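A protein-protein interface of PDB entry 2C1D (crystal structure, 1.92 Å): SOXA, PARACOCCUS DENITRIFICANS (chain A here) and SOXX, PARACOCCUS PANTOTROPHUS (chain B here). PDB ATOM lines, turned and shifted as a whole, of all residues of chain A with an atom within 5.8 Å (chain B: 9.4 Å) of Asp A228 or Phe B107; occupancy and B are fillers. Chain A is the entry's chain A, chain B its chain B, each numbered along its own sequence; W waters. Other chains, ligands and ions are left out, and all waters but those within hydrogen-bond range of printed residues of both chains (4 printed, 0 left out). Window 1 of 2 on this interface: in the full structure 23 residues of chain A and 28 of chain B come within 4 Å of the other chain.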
ATOM      1  N   LEU A 176      11.484 -13.332  24.088  1.00  0.00           N
ATOM      2  CA  LEU A 176      10.750 -13.438  22.833  1.00  0.00           C
ATOM      3  C   LEU A 176       9.964 -12.190  22.418  1.00  0.00           C
ATOM      4  O   LEU A 176       9.528 -12.118  21.271  1.00  0.00           O
ATOM      5  CB  LEU A 176       9.803 -14.658  22.864  1.00  0.00           C
ATOM      6  CG  LEU A 176      10.492 -16.020  22.878  1.00  0.00           C
ATOM      7  CD1 LEU A 176       9.499 -17.229  22.974  1.00  0.00           C
ATOM      8  CD2 LEU A 176      11.398 -16.162  21.667  1.00  0.00           C
ATOM      9  N   VAL A 223      -0.382 -17.683  33.796  1.00  0.00           N
ATOM     10  CA  VAL A 223       0.963 -17.927  34.299  1.00  0.00           C
ATOM     11  C   VAL A 223       1.872 -18.511  33.225  1.00  0.00           C
ATOM     12  O   VAL A 223       3.009 -18.015  32.989  1.00  0.00           O
ATOM     13  CB  VAL A 223       0.958 -18.901  35.517  1.00  0.00           C
ATOM     14  CG1 VAL A 223       2.346 -19.329  35.874  1.00  0.00           C
ATOM     15  CG2 VAL A 223       0.284 -18.256  36.738  1.00  0.00           C
ATOM     16  N   GLY A 224       1.359 -19.557  32.573  1.00  0.00           N
ATOM     17  CA  GLY A 224       2.046 -20.219  31.474  1.00  0.00           C
ATOM     18  C   GLY A 224       2.230 -19.369  30.217  1.00  0.00           C
ATOM     19  O   GLY A 224       3.298 -19.410  29.625  1.00  0.00           O
ATOM     20  N   CSS A 225       1.217 -18.599  29.816  1.00  0.00           N
ATOM     21  CA  CSS A 225       1.344 -17.766  28.645  1.00  0.00           C
ATOM     22  CB  CSS A 225       0.051 -17.002  28.419  1.00  0.00           C
ATOM     23  SG  CSS A 225      -1.370 -18.057  28.180  1.00  0.00           S
ATOM     24  SD  CSS A 225      -1.110 -18.763  26.340  1.00  0.00           S
ATOM     25  C   CSS A 225       2.468 -16.753  28.762  1.00  0.00           C
ATOM     26  O   CSS A 225       3.190 -16.515  27.790  1.00  0.00           O
ATOM     27  N   VAL A 226       2.624 -16.117  29.913  1.00  0.00           N
ATOM     28  CA  VAL A 226       3.730 -15.168  30.001  1.00  0.00           C
ATOM     29  C   VAL A 226       5.075 -15.849  30.191  1.00  0.00           C
ATOM     30  O   VAL A 226       6.041 -15.411  29.600  1.00  0.00           O
ATOM     31  CB  VAL A 226       3.501 -13.874  30.830  1.00  0.00           C
ATOM     32  CG1 VAL A 226       2.071 -13.697  31.347  1.00  0.00           C
ATOM     33  CG2 VAL A 226       4.597 -13.602  31.846  1.00  0.00           C
ATOM     34  N   ARG A 227       5.127 -16.945  30.932  1.00  0.00           N
ATOM     35  CA  ARG A 227       6.359 -17.700  31.102  1.00  0.00           C
ATOM     36  C   ARG A 227       6.967 -18.095  29.753  1.00  0.00           C
ATOM     37  O   ARG A 227       8.194 -18.033  29.531  1.00  0.00           O
ATOM     38  CB  ARG A 227       6.032 -18.945  31.920  1.00  0.00           C
ATOM     39  CG  ARG A 227       7.127 -19.973  32.103  1.00  0.00           C
ATOM     40  CD  ARG A 227       6.555 -21.277  32.684  1.00  0.00           C
ATOM     41  NE  ARG A 227       5.760 -21.930  31.639  1.00  0.00           N
ATOM     42  CZ  ARG A 227       4.691 -22.714  31.836  1.00  0.00           C
ATOM     43  NH1 ARG A 227       4.260 -23.008  33.047  1.00  0.00           N
ATOM     44  NH2 ARG A 227       4.046 -23.216  30.783  1.00  0.00           N
ATOM     45  N   ASP A 228       6.089 -18.510  28.858  1.00  0.00           N
ATOM     46  CA  ASP A 228       6.491 -19.072  27.580  1.00  0.00           C
ATOM     47  C   ASP A 228       6.936 -18.030  26.551  1.00  0.00           C
ATOM     48  O   ASP A 228       7.338 -18.387  25.463  1.00  0.00           O
ATOM     49  CB  ASP A 228       5.361 -19.940  27.043  1.00  0.00           C
ATOM     50  CG  ASP A 228       5.199 -21.231  27.841  1.00  0.00           C
ATOM     51  OD1 ASP A 228       6.107 -21.587  28.634  1.00  0.00           O
ATOM     52  OD2 ASP A 228       4.210 -21.940  27.727  1.00  0.00           O
ATOM     53  N   THR A 229       6.860 -16.747  26.892  1.00  0.00           N
ATOM     54  CA  THR A 229       7.577 -15.717  26.142  1.00  0.00           C
ATOM     55  C   THR A 229       9.061 -15.601  26.554  1.00  0.00           C
ATOM     56  O   THR A 229       9.749 -14.684  26.122  1.00  0.00           O
ATOM     57  CB  THR A 229       6.892 -14.345  26.323  1.00  0.00           C
ATOM     58  OG1 THR A 229       7.064 -13.868  27.669  1.00  0.00           O
ATOM     59  CG2 THR A 229       5.365 -14.412  26.077  1.00  0.00           C
ATOM     60  N   ARG A 230       9.551 -16.545  27.359  1.00  0.00           N
ATOM     61  CA  ARG A 230      10.852 -16.454  28.024  1.00  0.00           C
ATOM     62  C   ARG A 230      10.916 -15.240  28.958  1.00  0.00           C
ATOM     63  O   ARG A 230      11.848 -14.406  28.869  1.00  0.00           O
ATOM     64  CB  ARG A 230      12.015 -16.435  27.034  1.00  0.00           C
ATOM     65  CG  ARG A 230      12.098 -17.667  26.143  1.00  0.00           C
ATOM     66  CD  ARG A 230      13.192 -17.602  25.093  1.00  0.00           C
ATOM     67  NE  ARG A 230      14.421 -18.105  25.661  1.00  0.00           N
ATOM     68  CZ  ARG A 230      14.976 -19.276  25.390  1.00  0.00           C
ATOM     69  NH1 ARG A 230      14.497 -20.082  24.457  1.00  0.00           N
ATOM     70  NH2 ARG A 230      16.086 -19.599  26.017  1.00  0.00           N
ATOM     71  N   ALA A 231       9.928 -15.168  29.849  1.00  0.00           N
ATOM     72  CA  ALA A 231       9.791 -14.080  30.834  1.00  0.00           C
ATOM     73  C   ALA A 231       9.677 -14.593  32.255  1.00  0.00           C
ATOM     74  O   ALA A 231       9.314 -15.756  32.497  1.00  0.00           O
ATOM     75  CB  ALA A 231       8.538 -13.232  30.562  1.00  0.00           C
ATOM     76  N   ASN B  36      12.951 -27.313  18.317  1.00  0.00           N
ATOM     77  CA  ASN B  36      12.100 -26.401  19.090  1.00  0.00           C
ATOM     78  C   ASN B  36      12.843 -25.438  20.036  1.00  0.00           C
ATOM     79  O   ASN B  36      12.456 -24.288  20.206  1.00  0.00           O
ATOM     80  CB  ASN B  36      11.042 -27.196  19.875  1.00  0.00           C
ATOM     81  CG  ASN B  36      10.122 -28.014  18.968  1.00  0.00           C
ATOM     82  OD1 ASN B  36      10.239 -27.980  17.745  1.00  0.00           O
ATOM     83  ND2 ASN B  36       9.227 -28.787  19.576  1.00  0.00           N
ATOM     84  N   ALA B  37      13.914 -25.902  20.643  1.00  0.00           N
ATOM     85  CA  ALA B  37      14.591 -25.116  21.658  1.00  0.00           C
ATOM     86  C   ALA B  37      15.662 -24.254  21.022  1.00  0.00           C
ATOM     87  O   ALA B  37      16.313 -23.507  21.711  1.00  0.00           O
ATOM     88  CB  ALA B  37      15.218 -26.029  22.693  1.00  0.00           C
ATOM     89  N   LEU B  38      15.867 -24.385  19.713  1.00  0.00           N
ATOM     90  CA  LEU B  38      16.870 -23.584  19.024  1.00  0.00           C
ATOM     91  C   LEU B  38      16.180 -22.520  18.163  1.00  0.00           C
ATOM     92  O   LEU B  38      15.572 -21.609  18.708  1.00  0.00           O
ATOM     93  CB  LEU B  38      17.833 -24.495  18.258  1.00  0.00           C
ATOM     94  CG  LEU B  38      18.630 -25.493  19.114  1.00  0.00           C
ATOM     95  CD1 LEU B  38      19.489 -26.389  18.222  1.00  0.00           C
ATOM     96  CD2 LEU B  38      19.497 -24.765  20.198  1.00  0.00           C
ATOM     97  N   ASN B  40      13.569 -22.853  16.026  1.00  0.00           N
ATOM     98  CA  ASN B  40      12.124 -23.058  16.059  1.00  0.00           C
ATOM     99  C   ASN B  40      11.420 -22.264  14.952  1.00  0.00           C
ATOM    100  O   ASN B  40      10.289 -21.807  15.125  1.00  0.00           O
ATOM    101  CB  ASN B  40      11.584 -22.699  17.449  1.00  0.00           C
ATOM    102  CG  ASN B  40      10.200 -23.278  17.721  1.00  0.00           C
ATOM    103  OD1 ASN B  40       9.823 -24.324  17.188  1.00  0.00           O
ATOM    104  ND2 ASN B  40       9.446 -22.603  18.574  1.00  0.00           N
ATOM    105  N   PHE B  90       6.783  -9.513  14.791  1.00  0.00           N
ATOM    106  CA  PHE B  90       6.461 -10.586  15.737  1.00  0.00           C
ATOM    107  C   PHE B  90       7.652 -11.546  15.806  1.00  0.00           C
ATOM    108  O   PHE B  90       7.861 -12.206  16.814  1.00  0.00           O
ATOM    109  CB  PHE B  90       5.158 -11.275  15.262  1.00  0.00           C
ATOM    110  CG  PHE B  90       4.709 -12.459  16.082  1.00  0.00           C
ATOM    111  CD1 PHE B  90       4.729 -12.444  17.482  1.00  0.00           C
ATOM    112  CD2 PHE B  90       4.214 -13.585  15.439  1.00  0.00           C
ATOM    113  CE1 PHE B  90       4.273 -13.560  18.216  1.00  0.00           C
ATOM    114  CE2 PHE B  90       3.784 -14.716  16.173  1.00  0.00           C
ATOM    115  CZ  PHE B  90       3.799 -14.681  17.566  1.00  0.00           C
ATOM    116  N   PRO B  92      10.931 -12.927  16.770  1.00  0.00           N
ATOM    117  CA  PRO B  92      11.836 -12.579  17.859  1.00  0.00           C
ATOM    118  C   PRO B  92      13.278 -12.485  17.344  1.00  0.00           C
ATOM    119  O   PRO B  92      13.583 -12.984  16.271  1.00  0.00           O
ATOM    120  CB  PRO B  92      11.653 -13.737  18.845  1.00  0.00           C
ATOM    121  CG  PRO B  92      11.331 -14.945  17.934  1.00  0.00           C
ATOM    122  CD  PRO B  92      10.528 -14.348  16.802  1.00  0.00           C
ATOM    123  N   ARG B 102      10.410  -7.800  31.832  1.00  0.00           N
ATOM    124  CA  ARG B 102      10.379  -9.003  32.655  1.00  0.00           C
ATOM    125  C   ARG B 102      11.223 -10.107  32.046  1.00  0.00           C
ATOM    126  O   ARG B 102      10.717 -11.186  31.708  1.00  0.00           O
ATOM    127  CB  ARG B 102       8.944  -9.479  32.855  1.00  0.00           C
ATOM    128  CG  ARG B 102       8.043  -8.481  33.581  1.00  0.00           C
ATOM    129  CD  ARG B 102       6.700  -9.067  33.993  1.00  0.00           C
ATOM    130  NE  ARG B 102       6.770 -10.051  35.088  1.00  0.00           N
ATOM    131  CZ  ARG B 102       6.653  -9.778  36.383  1.00  0.00           C
ATOM    132  NH1 ARG B 102       6.734 -10.751  37.265  1.00  0.00           N
ATOM    133  NH2 ARG B 102       6.444  -8.555  36.817  1.00  0.00           N
ATOM    134  N   PRO B 103      12.526  -9.860  31.872  1.00  0.00           N
ATOM    135  CA  PRO B 103      13.376 -10.877  31.262  1.00  0.00           C
ATOM    136  C   PRO B 103      13.342 -12.144  32.097  1.00  0.00           C
ATOM    137  O   PRO B 103      13.406 -12.095  33.354  1.00  0.00           O
ATOM    138  CB  PRO B 103      14.776 -10.224  31.243  1.00  0.00           C
ATOM    139  CG  PRO B 103      14.736  -9.190  32.308  1.00  0.00           C
ATOM    140  CD  PRO B 103      13.300  -8.665  32.269  1.00  0.00           C
ATOM    141  N   GLY B 104      13.227 -13.275  31.410  1.00  0.00           N
ATOM    142  CA  GLY B 104      13.112 -14.560  32.076  1.00  0.00           C
ATOM    143  C   GLY B 104      14.378 -15.380  32.001  1.00  0.00           C
ATOM    144  O   GLY B 104      15.258 -15.111  31.200  1.00  0.00           O
ATOM    145  N   ASP B 105      14.465 -16.393  32.852  1.00  0.00           N
ATOM    146  CA  ASP B 105      15.552 -17.360  32.830  1.00  0.00           C
ATOM    147  C   ASP B 105      15.009 -18.591  32.097  1.00  0.00           C
ATOM    148  O   ASP B 105      14.327 -19.428  32.687  1.00  0.00           O
ATOM    149  CB  ASP B 105      15.960 -17.699  34.254  1.00  0.00           C
ATOM    150  CG  ASP B 105      16.925 -18.872  34.336  1.00  0.00           C
ATOM    151  OD1 ASP B 105      17.628 -19.166  33.336  1.00  0.00           O
ATOM    152  OD2 ASP B 105      17.043 -19.526  35.392  1.00  0.00           O
ATOM    153  N   GLY B 106      15.301 -18.686  30.803  1.00  0.00           N
ATOM    154  CA  GLY B 106      14.751 -19.741  29.972  1.00  0.00           C
ATOM    155  C   GLY B 106      13.225 -19.741  30.050  1.00  0.00           C
ATOM    156  O   GLY B 106      12.594 -18.697  29.958  1.00  0.00           O
ATOM    157  N   PHE B 107      12.646 -20.920  30.243  1.00  0.00           N
ATOM    158  CA  PHE B 107      11.209 -21.079  30.394  1.00  0.00           C
ATOM    159  C   PHE B 107      10.828 -21.374  31.838  1.00  0.00           C
ATOM    160  O   PHE B 107       9.739 -21.888  32.112  1.00  0.00           O
ATOM    161  CB  PHE B 107      10.698 -22.189  29.460  1.00  0.00           C
ATOM    162  CG  PHE B 107      10.901 -21.880  28.003  1.00  0.00           C
ATOM    163  CD1 PHE B 107      12.004 -22.373  27.320  1.00  0.00           C
ATOM    164  CD2 PHE B 107      10.010 -21.069  27.323  1.00  0.00           C
ATOM    165  CE1 PHE B 107      12.205 -22.075  25.966  1.00  0.00           C
ATOM    166  CE2 PHE B 107      10.210 -20.756  25.979  1.00  0.00           C
ATOM    167  CZ  PHE B 107      11.300 -21.252  25.302  1.00  0.00           C
ATOM    168  N   SER B 108      11.702 -21.024  32.771  1.00  0.00           N
ATOM    169  CA  SER B 108      11.471 -21.322  34.189  1.00  0.00           C
ATOM    170  C   SER B 108      10.363 -20.458  34.788  1.00  0.00           C
ATOM    171  O   SER B 108       9.733 -20.811  35.782  1.00  0.00           O
ATOM    172  CB  SER B 108      12.749 -21.122  34.975  1.00  0.00           C
ATOM    173  OG  SER B 108      13.064 -19.752  35.062  1.00  0.00           O
ATOM    174  N   GLY B 109      10.101 -19.326  34.164  1.00  0.00           N
ATOM    175  CA  GLY B 109       9.235 -18.343  34.757  1.00  0.00           C
ATOM    176  C   GLY B 109       9.896 -17.488  35.830  1.00  0.00           C
ATOM    177  O   GLY B 109       9.221 -16.642  36.431  1.00  0.00           O
ATOM    178  N   LYS B 110      11.187 -17.696  36.071  1.00  0.00           N
ATOM    179  CA  LYS B 110      11.932 -16.893  37.041  1.00  0.00           C
ATOM    180  C   LYS B 110      12.690 -15.765  36.327  1.00  0.00           C
ATOM    181  O   LYS B 110      12.926 -15.811  35.106  1.00  0.00           O
ATOM    182  CB  LYS B 110      12.897 -17.756  37.846  1.00  0.00           C
ATOM    183  CG  LYS B 110      12.295 -19.113  38.324  1.00  0.00           C
ATOM    184  CD  LYS B 110      11.307 -18.971  39.489  1.00  0.00           C
ATOM    185  CE  LYS B 110      10.519 -20.296  39.705  1.00  0.00           C
ATOM    186  NZ  LYS B 110      11.404 -21.430  40.133  1.00  0.00           N
ATOM    187  N   ALA B 111      13.058 -14.747  37.099  1.00  0.00           N
ATOM    188  CA  ALA B 111      13.808 -13.632  36.580  1.00  0.00           C
ATOM    189  C   ALA B 111      15.169 -14.125  36.103  1.00  0.00           C
ATOM    190  O   ALA B 111      15.841 -14.926  36.762  1.00  0.00           O
ATOM    191  CB  ALA B 111      13.974 -12.524  37.658  1.00  0.00           C
ATOM    192  N   GLY B 112      15.550 -13.629  34.939  1.00  0.00           N
ATOM    193  CA  GLY B 112      16.884 -13.809  34.387  1.00  0.00           C
ATOM    194  C   GLY B 112      17.578 -12.456  34.338  1.00  0.00           C
ATOM    195  O   GLY B 112      16.982 -11.463  33.892  1.00  0.00           O
ATOM    196  N   LEU B 116      21.168 -11.656  29.125  1.00  0.00           N
ATOM    197  CA  LEU B 116      20.824 -13.051  28.929  1.00  0.00           C
ATOM    198  C   LEU B 116      21.743 -13.708  27.908  1.00  0.00           C
ATOM    199  O   LEU B 116      22.308 -13.028  27.031  1.00  0.00           O
ATOM    200  CB  LEU B 116      19.398 -13.128  28.380  1.00  0.00           C
ATOM    201  CG  LEU B 116      18.193 -13.311  29.306  1.00  0.00           C
ATOM    202  CD1 LEU B 116      18.396 -12.830  30.729  1.00  0.00           C
ATOM    203  CD2 LEU B 116      16.929 -12.737  28.675  1.00  0.00           C
ATOM    204  N   ILE B 119      19.316 -16.420  22.231  1.00  0.00           N
ATOM    205  CA  ILE B 119      18.606 -17.668  21.962  1.00  0.00           C
ATOM    206  C   ILE B 119      19.471 -18.608  21.105  1.00  0.00           C
ATOM    207  O   ILE B 119      19.548 -19.804  21.348  1.00  0.00           O
ATOM    208  CB  ILE B 119      17.219 -17.387  21.304  1.00  0.00           C
ATOM    209  CG1 ILE B 119      16.338 -16.552  22.264  1.00  0.00           C
ATOM    210  CG2 ILE B 119      16.548 -18.725  20.859  1.00  0.00           C
ATOM    211  CD1 ILE B 119      15.147 -15.890  21.574  1.00  0.00           C
HETATM  212  O   HOH W   1      15.737 -23.241  24.829  1.00  0.00           O
HETATM  213  O   HOH W   2      11.207 -17.785  32.107  1.00  0.00           O
HETATM  214  O   HOH W   3       8.929 -10.816  18.878  1.00  0.00           O
HETATM  215  O   HOH W   4      15.248 -17.147  28.016  1.00  0.00           O
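Of the 19 printed residues of chain B, 7 touch a printed residue of chain A. Of the 10 printed residues of chain A, 5 touch a printed residue of chain B. Among the printed residues, no Asp or Glu carboxylate lies within 4 Å of a Lys or Arg side-chain nitrogen of the other chain.
Asp A228 touches just one residue of chain B: Phe B107. Of chain A, only Arg A227 (3.2 Å), Asp A228 (3.8 Å) and Arg A230 (3.4 Å) come within 4 Å of Phe B107. Of chain B, only Phe B107 (3.2 Å) and Gly B109 (3.7 Å) come within 4 Å of Arg A227. No residue of chain B comes within 4 Å of Thr A229. Of the printed residues of chain A, Gly B106 touches Arg A230. Of the printed residues of chain A, Gly B104 touches Arg A230 and Ala A231. Printed residues of chain A within 4 Å of Ile B119: Leu A176. Of the printed residues of chain A, Arg B102 touches Ala A231 (3.2 Å). Asn B36 touches none of the printed residues of chain A. The nearest printed residue of chain B that does not touch Arg A230 is Ile B119 (4.2 Å).
O of Leu A176 touches CB of Pro B92, at 3.6 Å. Leu A176 touches Ile B119 (CD2 to CD1, 3.8 Å). Phe B107 touches Arg A227 (O to CG, 3.2 Å). Arg A227 touches Gly B109 (CG to N, 3.7 Å). Asp A228 touches Phe B107 (O to CE2, 3.8 Å). Arg A230 touches Gly B106 (CA to O, 3.4 Å). Arg A230 touches Phe B107 (NH1 to CE1, 3.4 Å). CA of Ala A231 touches O of Arg B102 (3.2 Å). Ala A231 touches Gly B104 (C to CA, 3.4 Å). O of Ala A231 touches CA of Gly B109 (3.4 Å).
Water W4 bridges NE of Arg A230 and N of Gly B106. Water W3 lies within hydrogen-bond range of O of Phe B90 (2.7 Å) and O of Leu A176 (2.8 Å). Water W2 lies within hydrogen-bond range of the backbone carbonyl oxygen (O) of Gly B106 (2.7 Å), the backbone NH (N) of Gly B109 (2.8 Å), the backbone carbonyl oxygen (O) of Ala A231 (2.8 Å) and the backbone NH (N) of Ser B108 (3.3 Å). Water W1 bridges O of Ala B37 and NH1 of Arg A230.
O of Thr A229 lies within hydrogen-bond range of N of Leu A176 (3.0 Å). The guanidinium group (NE) of Arg A227 is in salt-bridge range of the side-chain carboxylate (OD1) of Asp A228, at 3.0 Å.
O of Arg A230 is in hydrogen-bond range of N of Gly B104 (3.1 Å).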
